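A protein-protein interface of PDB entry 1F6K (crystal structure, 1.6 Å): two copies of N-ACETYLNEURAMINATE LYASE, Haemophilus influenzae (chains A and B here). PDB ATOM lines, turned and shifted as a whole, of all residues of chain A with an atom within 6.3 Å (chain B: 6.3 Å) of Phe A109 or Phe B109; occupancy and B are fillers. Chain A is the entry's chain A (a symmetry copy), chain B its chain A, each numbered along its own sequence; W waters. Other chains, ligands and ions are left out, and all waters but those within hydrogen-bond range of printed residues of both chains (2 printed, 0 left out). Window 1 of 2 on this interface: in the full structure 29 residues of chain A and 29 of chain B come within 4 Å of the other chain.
Of the printed residues of chain B, Phe A109 touches Phe B109 and Tyr B110. Of chain A, only Phe A109 (3.8 Å) and Tyr A110 (3.5 Å) come within 4 Å of Phe B109. Printed residues of chain B within 4 Å of Val A83: Phe B52 (3.3 Å). Of the printed residues of chain B, Tyr A110 touches Phe B52 (3.4 Å), Phe B109 (3.5 Å) and Leu B141 (3.4 Å). Printed residues of chain B within 4 Å of Leu A141: Tyr B110 (3.4 Å). Ser A82 touches none of the printed residues of chain B. Lys B112 touches none of the printed residues of chain A. The nearest residue of chain A that does not touch Phe B109 is Val A83 (5.3 Å). The nearest printed residue of chain B that does not touch Phe A52 is Ser B82 (5.8 Å).
Phe A52 touches Val B83, and with the chains exchanged Val A83 touches Phe B52. Phe A52 touches Tyr B110, and with the chains exchanged Tyr A110 touches Phe B52. Phe A52 touches Tyr B111, and with the chains exchanged Tyr A111 touches Phe B52. Phe A109 touches its own counterpart, Phe B109. Positions printed for both chains: 52, 81, 82, 83, 106, 107, 108, 109, 110, 111, 112, 113, 141, 142 and 144. Of the 11 pairs that touch across the chains among the printed residues, 11 have their exchanged pair printed and touching as well.
O of Phe A52 touches CG1 of Val B83, 3.3 Å away. CD2 of Phe A52 touches CE2 of Tyr B110 (3.4 Å). Phe A52 touches Tyr B111 (N to OH, 3.6 Å). Phe B52 touches Val A83 (O to CG1, 3.3 Å). CE2 of Phe A109 touches CE2 of Phe B109, 3.8 Å away. Phe A109 touches Tyr B110 (CE2 to CD1, 3.5 Å). CE2 of Tyr A110 touches CD2 of Phe B52 (3.4 Å). Leu B141 touches Tyr A110. OH of Tyr A111 touches N of Phe B52, at 3.6 Å. Tyr B110 touches Leu A141 (O to CD2, 3.4 Å).
Water W2 lies within hydrogen-bond range of the side-chain amino group of Lys A112 (2.7 Å), the backbone carbonyl oxygen of Tyr A110 (2.8 Å) and the backbone carbonyl oxygen of Leu B141 (2.9 Å). Water W1 lies within hydrogen-bond range of the side-chain amino group (NZ) of Lys B112, the backbone carbonyl oxygen (O) of Tyr B110 and the backbone carbonyl oxygen (O) of Leu A141.
Of the 15 printed residues of chain B, 6 touch a printed residue of chain A. Printed residues of chain B that touch a printed residue of chain A: Phe B52, Val B83, Phe B109, Tyr B110, Tyr B111 and Leu B141. Hydrophobic or aromatic side chains of chain B that line the printed part of chain A: Phe B52, Val B83, Phe B109, Tyr B110, Tyr B111 and Leu B141. Hydrophobic or aromatic side chains of chain A that line the printed part of chain B: Phe A52, Val A83, Phe A109, Tyr A110, Tyr A111 and Leu A141. Among the printed residues, 11 pairs touch across the chains. Among the printed residues, no Asp or Glu carboxylate lies within 4 Å of a Lys or Arg side-chain nitrogen of the other chain.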
ATOM      1  N   PHE A  52       6.268  10.808   0.151  1.00  0.00           N
ATOM      2  CA  PHE A  52       7.342  11.573  -0.469  1.00  0.00           C
ATOM      3  C   PHE A  52       8.294  10.792  -1.334  1.00  0.00           C
ATOM      4  O   PHE A  52       9.070  11.390  -2.094  1.00  0.00           O
ATOM      5  CB  PHE A  52       7.991  12.486   0.601  1.00  0.00           C
ATOM      6  CG  PHE A  52       6.931  13.386   1.188  1.00  0.00           C
ATOM      7  CD1 PHE A  52       6.500  14.516   0.536  1.00  0.00           C
ATOM      8  CD2 PHE A  52       6.357  13.061   2.419  1.00  0.00           C
ATOM      9  CE1 PHE A  52       5.515  15.326   1.081  1.00  0.00           C
ATOM     10  CE2 PHE A  52       5.365  13.859   2.969  1.00  0.00           C
ATOM     11  CZ  PHE A  52       4.959  15.000   2.302  1.00  0.00           C
ATOM     12  N   GLY A  81       0.688  18.231   0.221  1.00  0.00           N
ATOM     13  CA  GLY A  81       1.851  19.096   0.257  1.00  0.00           C
ATOM     14  C   GLY A  81       3.061  18.469  -0.434  1.00  0.00           C
ATOM     15  O   GLY A  81       3.278  17.260  -0.435  1.00  0.00           O
ATOM     16  N   SER A  82       3.858  19.354  -1.025  1.00  0.00           N
ATOM     17  CA  SER A  82       5.067  18.942  -1.764  1.00  0.00           C
ATOM     18  C   SER A  82       5.960  20.176  -1.863  1.00  0.00           C
ATOM     19  O   SER A  82       5.517  21.290  -1.572  1.00  0.00           O
ATOM     20  CB  SER A  82       4.591  18.592  -3.178  1.00  0.00           C
ATOM     21  OG  SER A  82       5.651  18.348  -4.075  1.00  0.00           O
ATOM     22  N   VAL A  83       7.172  20.023  -2.373  1.00  0.00           N
ATOM     23  CA  VAL A  83       8.092  21.135  -2.638  1.00  0.00           C
ATOM     24  C   VAL A  83       7.677  21.696  -3.996  1.00  0.00           C
ATOM     25  O   VAL A  83       7.928  22.876  -4.264  1.00  0.00           O
ATOM     26  CB  VAL A  83       9.557  20.652  -2.714  1.00  0.00           C
ATOM     27  CG1 VAL A  83      10.531  21.800  -3.064  1.00  0.00           C
ATOM     28  CG2 VAL A  83      10.057  19.995  -1.431  1.00  0.00           C
ATOM     29  N   VAL A 106       2.130  19.711   4.063  1.00  0.00           N
ATOM     30  CA  VAL A 106       3.386  19.955   4.799  1.00  0.00           C
ATOM     31  C   VAL A 106       3.958  21.314   4.391  1.00  0.00           C
ATOM     32  O   VAL A 106       3.771  21.786   3.265  1.00  0.00           O
ATOM     33  CB  VAL A 106       4.387  18.827   4.502  1.00  0.00           C
ATOM     34  CG1 VAL A 106       4.868  18.849   3.048  1.00  0.00           C
ATOM     35  CG2 VAL A 106       5.538  18.909   5.492  1.00  0.00           C
ATOM     36  N   THR A 107       4.638  21.967   5.337  1.00  0.00           N
ATOM     37  CA  THR A 107       5.330  23.228   4.952  1.00  0.00           C
ATOM     38  C   THR A 107       6.317  22.874   3.853  1.00  0.00           C
ATOM     39  O   THR A 107       6.975  21.830   3.930  1.00  0.00           O
ATOM     40  CB  THR A 107       6.042  23.717   6.224  1.00  0.00           C
ATOM     41  OG1 THR A 107       6.747  22.597   6.791  1.00  0.00           O
ATOM     42  CG2 THR A 107       5.078  24.159   7.320  1.00  0.00           C
ATOM     43  N   PRO A 108       6.418  23.646   2.775  1.00  0.00           N
ATOM     44  CA  PRO A 108       7.360  23.365   1.698  1.00  0.00           C
ATOM     45  C   PRO A 108       8.749  23.159   2.293  1.00  0.00           C
ATOM     46  O   PRO A 108       9.138  23.950   3.155  1.00  0.00           O
ATOM     47  CB  PRO A 108       7.266  24.546   0.759  1.00  0.00           C
ATOM     48  CG  PRO A 108       6.390  25.552   1.407  1.00  0.00           C
ATOM     49  CD  PRO A 108       5.720  24.934   2.601  1.00  0.00           C
ATOM     50  N   PHE A 109       9.467  22.121   1.871  1.00  0.00           N
ATOM     51  CA  PHE A 109      10.767  21.833   2.482  1.00  0.00           C
ATOM     52  C   PHE A 109      11.936  21.818   1.514  1.00  0.00           C
ATOM     53  O   PHE A 109      11.843  22.287   0.382  1.00  0.00           O
ATOM     54  CB  PHE A 109      10.665  20.513   3.267  1.00  0.00           C
ATOM     55  CG  PHE A 109      10.199  19.345   2.455  1.00  0.00           C
ATOM     56  CD1 PHE A 109       8.852  19.120   2.193  1.00  0.00           C
ATOM     57  CD2 PHE A 109      11.100  18.455   1.889  1.00  0.00           C
ATOM     58  CE1 PHE A 109       8.422  18.048   1.432  1.00  0.00           C
ATOM     59  CE2 PHE A 109      10.690  17.380   1.139  1.00  0.00           C
ATOM     60  CZ  PHE A 109       9.342  17.173   0.894  1.00  0.00           C
ATOM     61  N   TYR A 110      13.086  21.326   1.959  1.00  0.00           N
ATOM     62  CA  TYR A 110      14.327  21.246   1.202  1.00  0.00           C
ATOM     63  C   TYR A 110      14.920  22.653   1.089  1.00  0.00           C
ATOM     64  O   TYR A 110      15.879  22.980   1.812  1.00  0.00           O
ATOM     65  CB  TYR A 110      14.205  20.577  -0.163  1.00  0.00           C
ATOM     66  CG  TYR A 110      15.577  20.387  -0.792  1.00  0.00           C
ATOM     67  CD1 TYR A 110      16.401  19.346  -0.379  1.00  0.00           C
ATOM     68  CD2 TYR A 110      16.044  21.283  -1.744  1.00  0.00           C
ATOM     69  CE1 TYR A 110      17.659  19.186  -0.940  1.00  0.00           C
ATOM     70  CE2 TYR A 110      17.313  21.128  -2.296  1.00  0.00           C
ATOM     71  CZ  TYR A 110      18.103  20.085  -1.886  1.00  0.00           C
ATOM     72  OH  TYR A 110      19.369  19.928  -2.426  1.00  0.00           O
ATOM     73  N   TYR A 111      14.368  23.498   0.233  1.00  0.00           N
ATOM     74  CA  TYR A 111      14.808  24.891   0.175  1.00  0.00           C
ATOM     75  C   TYR A 111      14.361  25.600   1.458  1.00  0.00           C
ATOM     76  O   TYR A 111      13.375  25.198   2.099  1.00  0.00           O
ATOM     77  CB  TYR A 111      14.182  25.633  -1.008  1.00  0.00           C
ATOM     78  CG  TYR A 111      14.635  25.071  -2.338  1.00  0.00           C
ATOM     79  CD1 TYR A 111      15.906  25.353  -2.816  1.00  0.00           C
ATOM     80  CD2 TYR A 111      13.807  24.266  -3.106  1.00  0.00           C
ATOM     81  CE1 TYR A 111      16.340  24.853  -4.029  1.00  0.00           C
ATOM     82  CE2 TYR A 111      14.244  23.748  -4.311  1.00  0.00           C
ATOM     83  CZ  TYR A 111      15.503  24.055  -4.776  1.00  0.00           C
ATOM     84  OH  TYR A 111      15.936  23.537  -5.979  1.00  0.00           O
ATOM     85  N   LYS A 112      15.030  26.685   1.815  1.00  0.00           N
ATOM     86  CA  LYS A 112      14.678  27.446   3.007  1.00  0.00           C
ATOM     87  C   LYS A 112      13.716  28.573   2.660  1.00  0.00           C
ATOM     88  O   LYS A 112      14.107  29.743   2.628  1.00  0.00           O
ATOM     89  CB  LYS A 112      15.929  28.017   3.682  1.00  0.00           C
ATOM     90  CG  LYS A 112      16.957  26.997   4.139  1.00  0.00           C
ATOM     91  CD  LYS A 112      16.380  25.921   5.059  1.00  0.00           C
ATOM     92  CE  LYS A 112      17.490  25.115   5.707  1.00  0.00           C
ATOM     93  NZ  LYS A 112      16.969  24.016   6.579  1.00  0.00           N
ATOM     94  N   PHE A 113      12.438  28.262   2.511  1.00  0.00           N
ATOM     95  CA  PHE A 113      11.433  29.246   2.168  1.00  0.00           C
ATOM     96  C   PHE A 113      11.142  30.289   3.232  1.00  0.00           C
ATOM     97  O   PHE A 113      11.184  29.965   4.425  1.00  0.00           O
ATOM     98  CB  PHE A 113      10.125  28.493   1.845  1.00  0.00           C
ATOM     99  CG  PHE A 113      10.273  27.610   0.637  1.00  0.00           C
ATOM    100  CD1 PHE A 113      10.197  28.142  -0.641  1.00  0.00           C
ATOM    101  CD2 PHE A 113      10.485  26.247   0.772  1.00  0.00           C
ATOM    102  CE1 PHE A 113      10.332  27.330  -1.756  1.00  0.00           C
ATOM    103  CE2 PHE A 113      10.608  25.428  -0.340  1.00  0.00           C
ATOM    104  CZ  PHE A 113      10.522  25.965  -1.607  1.00  0.00           C
ATOM    105  N   LEU A 141      11.419  16.553  10.598  1.00  0.00           N
ATOM    106  CA  LEU A 141      11.756  16.200   9.222  1.00  0.00           C
ATOM    107  C   LEU A 141      11.985  17.432   8.357  1.00  0.00           C
ATOM    108  O   LEU A 141      12.882  17.404   7.501  1.00  0.00           O
ATOM    109  CB  LEU A 141      10.659  15.323   8.615  1.00  0.00           C
ATOM    110  CG  LEU A 141      10.414  13.973   9.304  1.00  0.00           C
ATOM    111  CD1 LEU A 141       9.438  13.132   8.481  1.00  0.00           C
ATOM    112  CD2 LEU A 141      11.705  13.202   9.535  1.00  0.00           C
ATOM    113  N   THR A 142      11.184  18.481   8.533  1.00  0.00           N
ATOM    114  CA  THR A 142      11.308  19.644   7.675  1.00  0.00           C
ATOM    115  C   THR A 142      12.397  20.623   8.082  1.00  0.00           C
ATOM    116  O   THR A 142      13.017  21.231   7.208  1.00  0.00           O
ATOM    117  CB  THR A 142       9.989  20.452   7.599  1.00  0.00           C
ATOM    118  OG1 THR A 142       9.691  20.969   8.899  1.00  0.00           O
ATOM    119  CG2 THR A 142       8.838  19.556   7.154  1.00  0.00           C
ATOM    120  N   VAL A 144      11.515  23.272   9.713  1.00  0.00           N
ATOM    121  CA  VAL A 144      10.735  24.497   9.729  1.00  0.00           C
ATOM    122  C   VAL A 144       9.990  24.624  11.058  1.00  0.00           C
ATOM    123  O   VAL A 144       9.241  23.722  11.411  1.00  0.00           O
ATOM    124  CB  VAL A 144       9.709  24.541   8.580  1.00  0.00           C
ATOM    125  CG1 VAL A 144       8.972  25.872   8.540  1.00  0.00           C
ATOM    126  CG2 VAL A 144      10.379  24.272   7.241  1.00  0.00           C
ATOM    127  N   PHE B  52      14.116  20.780  -7.366  1.00  0.00           N
ATOM    128  CA  PHE B  52      13.214  20.113  -6.436  1.00  0.00           C
ATOM    129  C   PHE B  52      11.800  20.631  -6.403  1.00  0.00           C
ATOM    130  O   PHE B  52      10.914  19.969  -5.842  1.00  0.00           O
ATOM    131  CB  PHE B  52      13.918  19.977  -5.064  1.00  0.00           C
ATOM    132  CG  PHE B  52      15.203  19.206  -5.245  1.00  0.00           C
ATOM    133  CD1 PHE B  52      15.216  17.835  -5.349  1.00  0.00           C
ATOM    134  CD2 PHE B  52      16.414  19.897  -5.326  1.00  0.00           C
ATOM    135  CE1 PHE B  52      16.403  17.141  -5.529  1.00  0.00           C
ATOM    136  CE2 PHE B  52      17.606  19.213  -5.515  1.00  0.00           C
ATOM    137  CZ  PHE B  52      17.596  17.833  -5.600  1.00  0.00           C
ATOM    138  N   GLY B  81      19.174  13.058  -8.378  1.00  0.00           N
ATOM    139  CA  GLY B  81      18.763  12.624  -7.057  1.00  0.00           C
ATOM    140  C   GLY B  81      17.380  13.151  -6.678  1.00  0.00           C
ATOM    141  O   GLY B  81      16.955  14.241  -7.053  1.00  0.00           O
ATOM    142  N   SER B  82      16.687  12.326  -5.900  1.00  0.00           N
ATOM    143  CA  SER B  82      15.321  12.648  -5.445  1.00  0.00           C
ATOM    144  C   SER B  82      15.048  11.770  -4.226  1.00  0.00           C
ATOM    145  O   SER B  82      15.805  10.836  -3.951  1.00  0.00           O
ATOM    146  CB  SER B  82      14.389  12.190  -6.572  1.00  0.00           C
ATOM    147  OG  SER B  82      13.024  12.260  -6.226  1.00  0.00           O
ATOM    148  N   VAL B  83      13.924  11.974  -3.556  1.00  0.00           N
ATOM    149  CA  VAL B  83      13.475  11.131  -2.441  1.00  0.00           C
ATOM    150  C   VAL B  83      12.781   9.934  -3.086  1.00  0.00           C
ATOM    151  O   VAL B  83      12.723   8.865  -2.469  1.00  0.00           O
ATOM    152  CB  VAL B  83      12.469  11.877  -1.539  1.00  0.00           C
ATOM    153  CG1 VAL B  83      11.931  10.980  -0.401  1.00  0.00           C
ATOM    154  CG2 VAL B  83      13.032  13.145  -0.903  1.00  0.00           C
ATOM    155  N   VAL B 106      21.756  13.885  -4.959  1.00  0.00           N
ATOM    156  CA  VAL B 106      21.687  14.322  -3.551  1.00  0.00           C
ATOM    157  C   VAL B 106      21.383  13.117  -2.659  1.00  0.00           C
ATOM    158  O   VAL B 106      20.720  12.158  -3.067  1.00  0.00           O
ATOM    159  CB  VAL B 106      20.607  15.405  -3.397  1.00  0.00           C
ATOM    160  CG1 VAL B 106      19.197  14.851  -3.621  1.00  0.00           C
ATOM    161  CG2 VAL B 106      20.757  16.069  -2.038  1.00  0.00           C
ATOM    162  N   THR B 107      21.908  13.155  -1.431  1.00  0.00           N
ATOM    163  CA  THR B 107      21.530  12.074  -0.480  1.00  0.00           C
ATOM    164  C   THR B 107      20.020  12.129  -0.325  1.00  0.00           C
ATOM    165  O   THR B 107      19.449  13.222  -0.245  1.00  0.00           O
ATOM    166  CB  THR B 107      22.252  12.408   0.837  1.00  0.00           C
ATOM    167  OG1 THR B 107      22.021  13.799   1.125  1.00  0.00           O
ATOM    168  CG2 THR B 107      23.769  12.283   0.738  1.00  0.00           C
ATOM    169  N   PRO B 108      19.308  11.005  -0.350  1.00  0.00           N
ATOM    170  CA  PRO B 108      17.858  10.996  -0.188  1.00  0.00           C
ATOM    171  C   PRO B 108      17.492  11.788   1.062  1.00  0.00           C
ATOM    172  O   PRO B 108      18.148  11.597   2.088  1.00  0.00           O
ATOM    173  CB  PRO B 108      17.468   9.537  -0.123  1.00  0.00           C
ATOM    174  CG  PRO B 108      18.723   8.748  -0.086  1.00  0.00           C
ATOM    175  CD  PRO B 108      19.887   9.649  -0.391  1.00  0.00           C
ATOM    176  N   PHE B 109      16.495  12.667   0.981  1.00  0.00           N
ATOM    177  CA  PHE B 109      16.171  13.514   2.132  1.00  0.00           C
ATOM    178  C   PHE B 109      14.747  13.383   2.638  1.00  0.00           C
ATOM    179  O   PHE B 109      14.025  12.446   2.301  1.00  0.00           O
ATOM    180  CB  PHE B 109      16.516  14.973   1.785  1.00  0.00           C
ATOM    181  CG  PHE B 109      15.848  15.491   0.550  1.00  0.00           C
ATOM    182  CD1 PHE B 109      16.345  15.228  -0.722  1.00  0.00           C
ATOM    183  CD2 PHE B 109      14.672  16.224   0.619  1.00  0.00           C
ATOM    184  CE1 PHE B 109      15.721  15.695  -1.864  1.00  0.00           C
ATOM    185  CE2 PHE B 109      14.044  16.703  -0.505  1.00  0.00           C
ATOM    186  CZ  PHE B 109      14.559  16.432  -1.761  1.00  0.00           C
ATOM    187  N   TYR B 110      14.325  14.292   3.507  1.00  0.00           N
ATOM    188  CA  TYR B 110      13.009  14.329   4.130  1.00  0.00           C
ATOM    189  C   TYR B 110      12.938  13.222   5.185  1.00  0.00           C
ATOM    190  O   TYR B 110      13.048  13.508   6.391  1.00  0.00           O
ATOM    191  CB  TYR B 110      11.837  14.257   3.158  1.00  0.00           C
ATOM    192  CG  TYR B 110      10.520  14.478   3.888  1.00  0.00           C
ATOM    193  CD1 TYR B 110      10.120  15.762   4.240  1.00  0.00           C
ATOM    194  CD2 TYR B 110       9.732  13.398   4.259  1.00  0.00           C
ATOM    195  CE1 TYR B 110       8.929  15.960   4.922  1.00  0.00           C
ATOM    196  CE2 TYR B 110       8.544  13.598   4.956  1.00  0.00           C
ATOM    197  CZ  TYR B 110       8.159  14.874   5.280  1.00  0.00           C
ATOM    198  OH  TYR B 110       6.981  15.082   5.978  1.00  0.00           O
ATOM    199  N   TYR B 111      12.787  11.974   4.772  1.00  0.00           N
ATOM    200  CA  TYR B 111      12.841  10.864   5.722  1.00  0.00           C
ATOM    201  C   TYR B 111      14.281  10.724   6.230  1.00  0.00           C
ATOM    202  O   TYR B 111      15.241  11.111   5.542  1.00  0.00           O
ATOM    203  CB  TYR B 111      12.449   9.538   5.067  1.00  0.00           C
ATOM    204  CG  TYR B 111      11.007   9.533   4.610  1.00  0.00           C
ATOM    205  CD1 TYR B 111       9.983   9.393   5.537  1.00  0.00           C
ATOM    206  CD2 TYR B 111      10.668   9.668   3.273  1.00  0.00           C
ATOM    207  CE1 TYR B 111       8.660   9.382   5.143  1.00  0.00           C
ATOM    208  CE2 TYR B 111       9.343   9.677   2.876  1.00  0.00           C
ATOM    209  CZ  TYR B 111       8.344   9.519   3.811  1.00  0.00           C
ATOM    210  OH  TYR B 111       7.023   9.528   3.411  1.00  0.00           O
ATOM    211  N   LYS B 112      14.456  10.123   7.397  1.00  0.00           N
ATOM    212  CA  LYS B 112      15.783   9.921   7.964  1.00  0.00           C
ATOM    213  C   LYS B 112      16.334   8.559   7.570  1.00  0.00           C
ATOM    214  O   LYS B 112      16.382   7.640   8.392  1.00  0.00           O
ATOM    215  CB  LYS B 112      15.751  10.051   9.490  1.00  0.00           C
ATOM    216  CG  LYS B 112      15.276  11.387  10.031  1.00  0.00           C
ATOM    217  CD  LYS B 112      16.056  12.579   9.478  1.00  0.00           C
ATOM    218  CE  LYS B 112      15.739  13.841  10.260  1.00  0.00           C
ATOM    219  NZ  LYS B 112      16.444  15.045   9.721  1.00  0.00           N
ATOM    220  N   PHE B 113      16.860   8.438   6.361  1.00  0.00           N
ATOM    221  CA  PHE B 113      17.402   7.189   5.869  1.00  0.00           C
ATOM    222  C   PHE B 113      18.665   6.704   6.559  1.00  0.00           C
ATOM    223  O   PHE B 113      19.499   7.531   6.948  1.00  0.00           O
ATOM    224  CB  PHE B 113      17.698   7.362   4.365  1.00  0.00           C
ATOM    225  CG  PHE B 113      16.443   7.610   3.574  1.00  0.00           C
ATOM    226  CD1 PHE B 113      15.613   6.558   3.217  1.00  0.00           C
ATOM    227  CD2 PHE B 113      16.089   8.891   3.183  1.00  0.00           C
ATOM    228  CE1 PHE B 113      14.456   6.784   2.488  1.00  0.00           C
ATOM    229  CE2 PHE B 113      14.938   9.122   2.443  1.00  0.00           C
ATOM    230  CZ  PHE B 113      14.124   8.068   2.085  1.00  0.00           C
ATOM    231  N   LEU B 141      20.871  21.863   3.674  1.00  0.00           N
ATOM    232  CA  LEU B 141      19.509  21.629   3.201  1.00  0.00           C
ATOM    233  C   LEU B 141      19.007  20.240   3.574  1.00  0.00           C
ATOM    234  O   LEU B 141      17.821  20.103   3.907  1.00  0.00           O
ATOM    235  CB  LEU B 141      19.430  21.831   1.686  1.00  0.00           C
ATOM    236  CG  LEU B 141      19.773  23.238   1.174  1.00  0.00           C
ATOM    237  CD1 LEU B 141      19.466  23.342  -0.319  1.00  0.00           C
ATOM    238  CD2 LEU B 141      19.034  24.325   1.939  1.00  0.00           C
ATOM    239  N   THR B 142      19.860  19.221   3.490  1.00  0.00           N
ATOM    240  CA  THR B 142      19.406  17.869   3.752  1.00  0.00           C
ATOM    241  C   THR B 142      19.357  17.486   5.223  1.00  0.00           C
ATOM    242  O   THR B 142      18.471  16.726   5.618  1.00  0.00           O
ATOM    243  CB  THR B 142      20.292  16.813   3.047  1.00  0.00           C
ATOM    244  OG1 THR B 142      21.612  16.882   3.593  1.00  0.00           O
ATOM    245  CG2 THR B 142      20.367  17.091   1.549  1.00  0.00           C
ATOM    246  N   VAL B 144      21.800  15.733   6.410  1.00  0.00           N
ATOM    247  CA  VAL B 144      22.560  14.495   6.356  1.00  0.00           C
ATOM    248  C   VAL B 144      24.057  14.801   6.386  1.00  0.00           C
ATOM    249  O   VAL B 144      24.532  15.545   5.537  1.00  0.00           O
ATOM    250  CB  VAL B 144      22.245  13.683   5.085  1.00  0.00           C
ATOM    251  CG1 VAL B 144      22.962  12.341   5.089  1.00  0.00           C
ATOM    252  CG2 VAL B 144      20.746  13.476   4.928  1.00  0.00           C
HETATM  253  O   HOH W   1      14.884  15.313   7.528  1.00  0.00           O
HETATM  254  O   HOH W   2      16.190  22.406   4.550  1.00  0.00           O
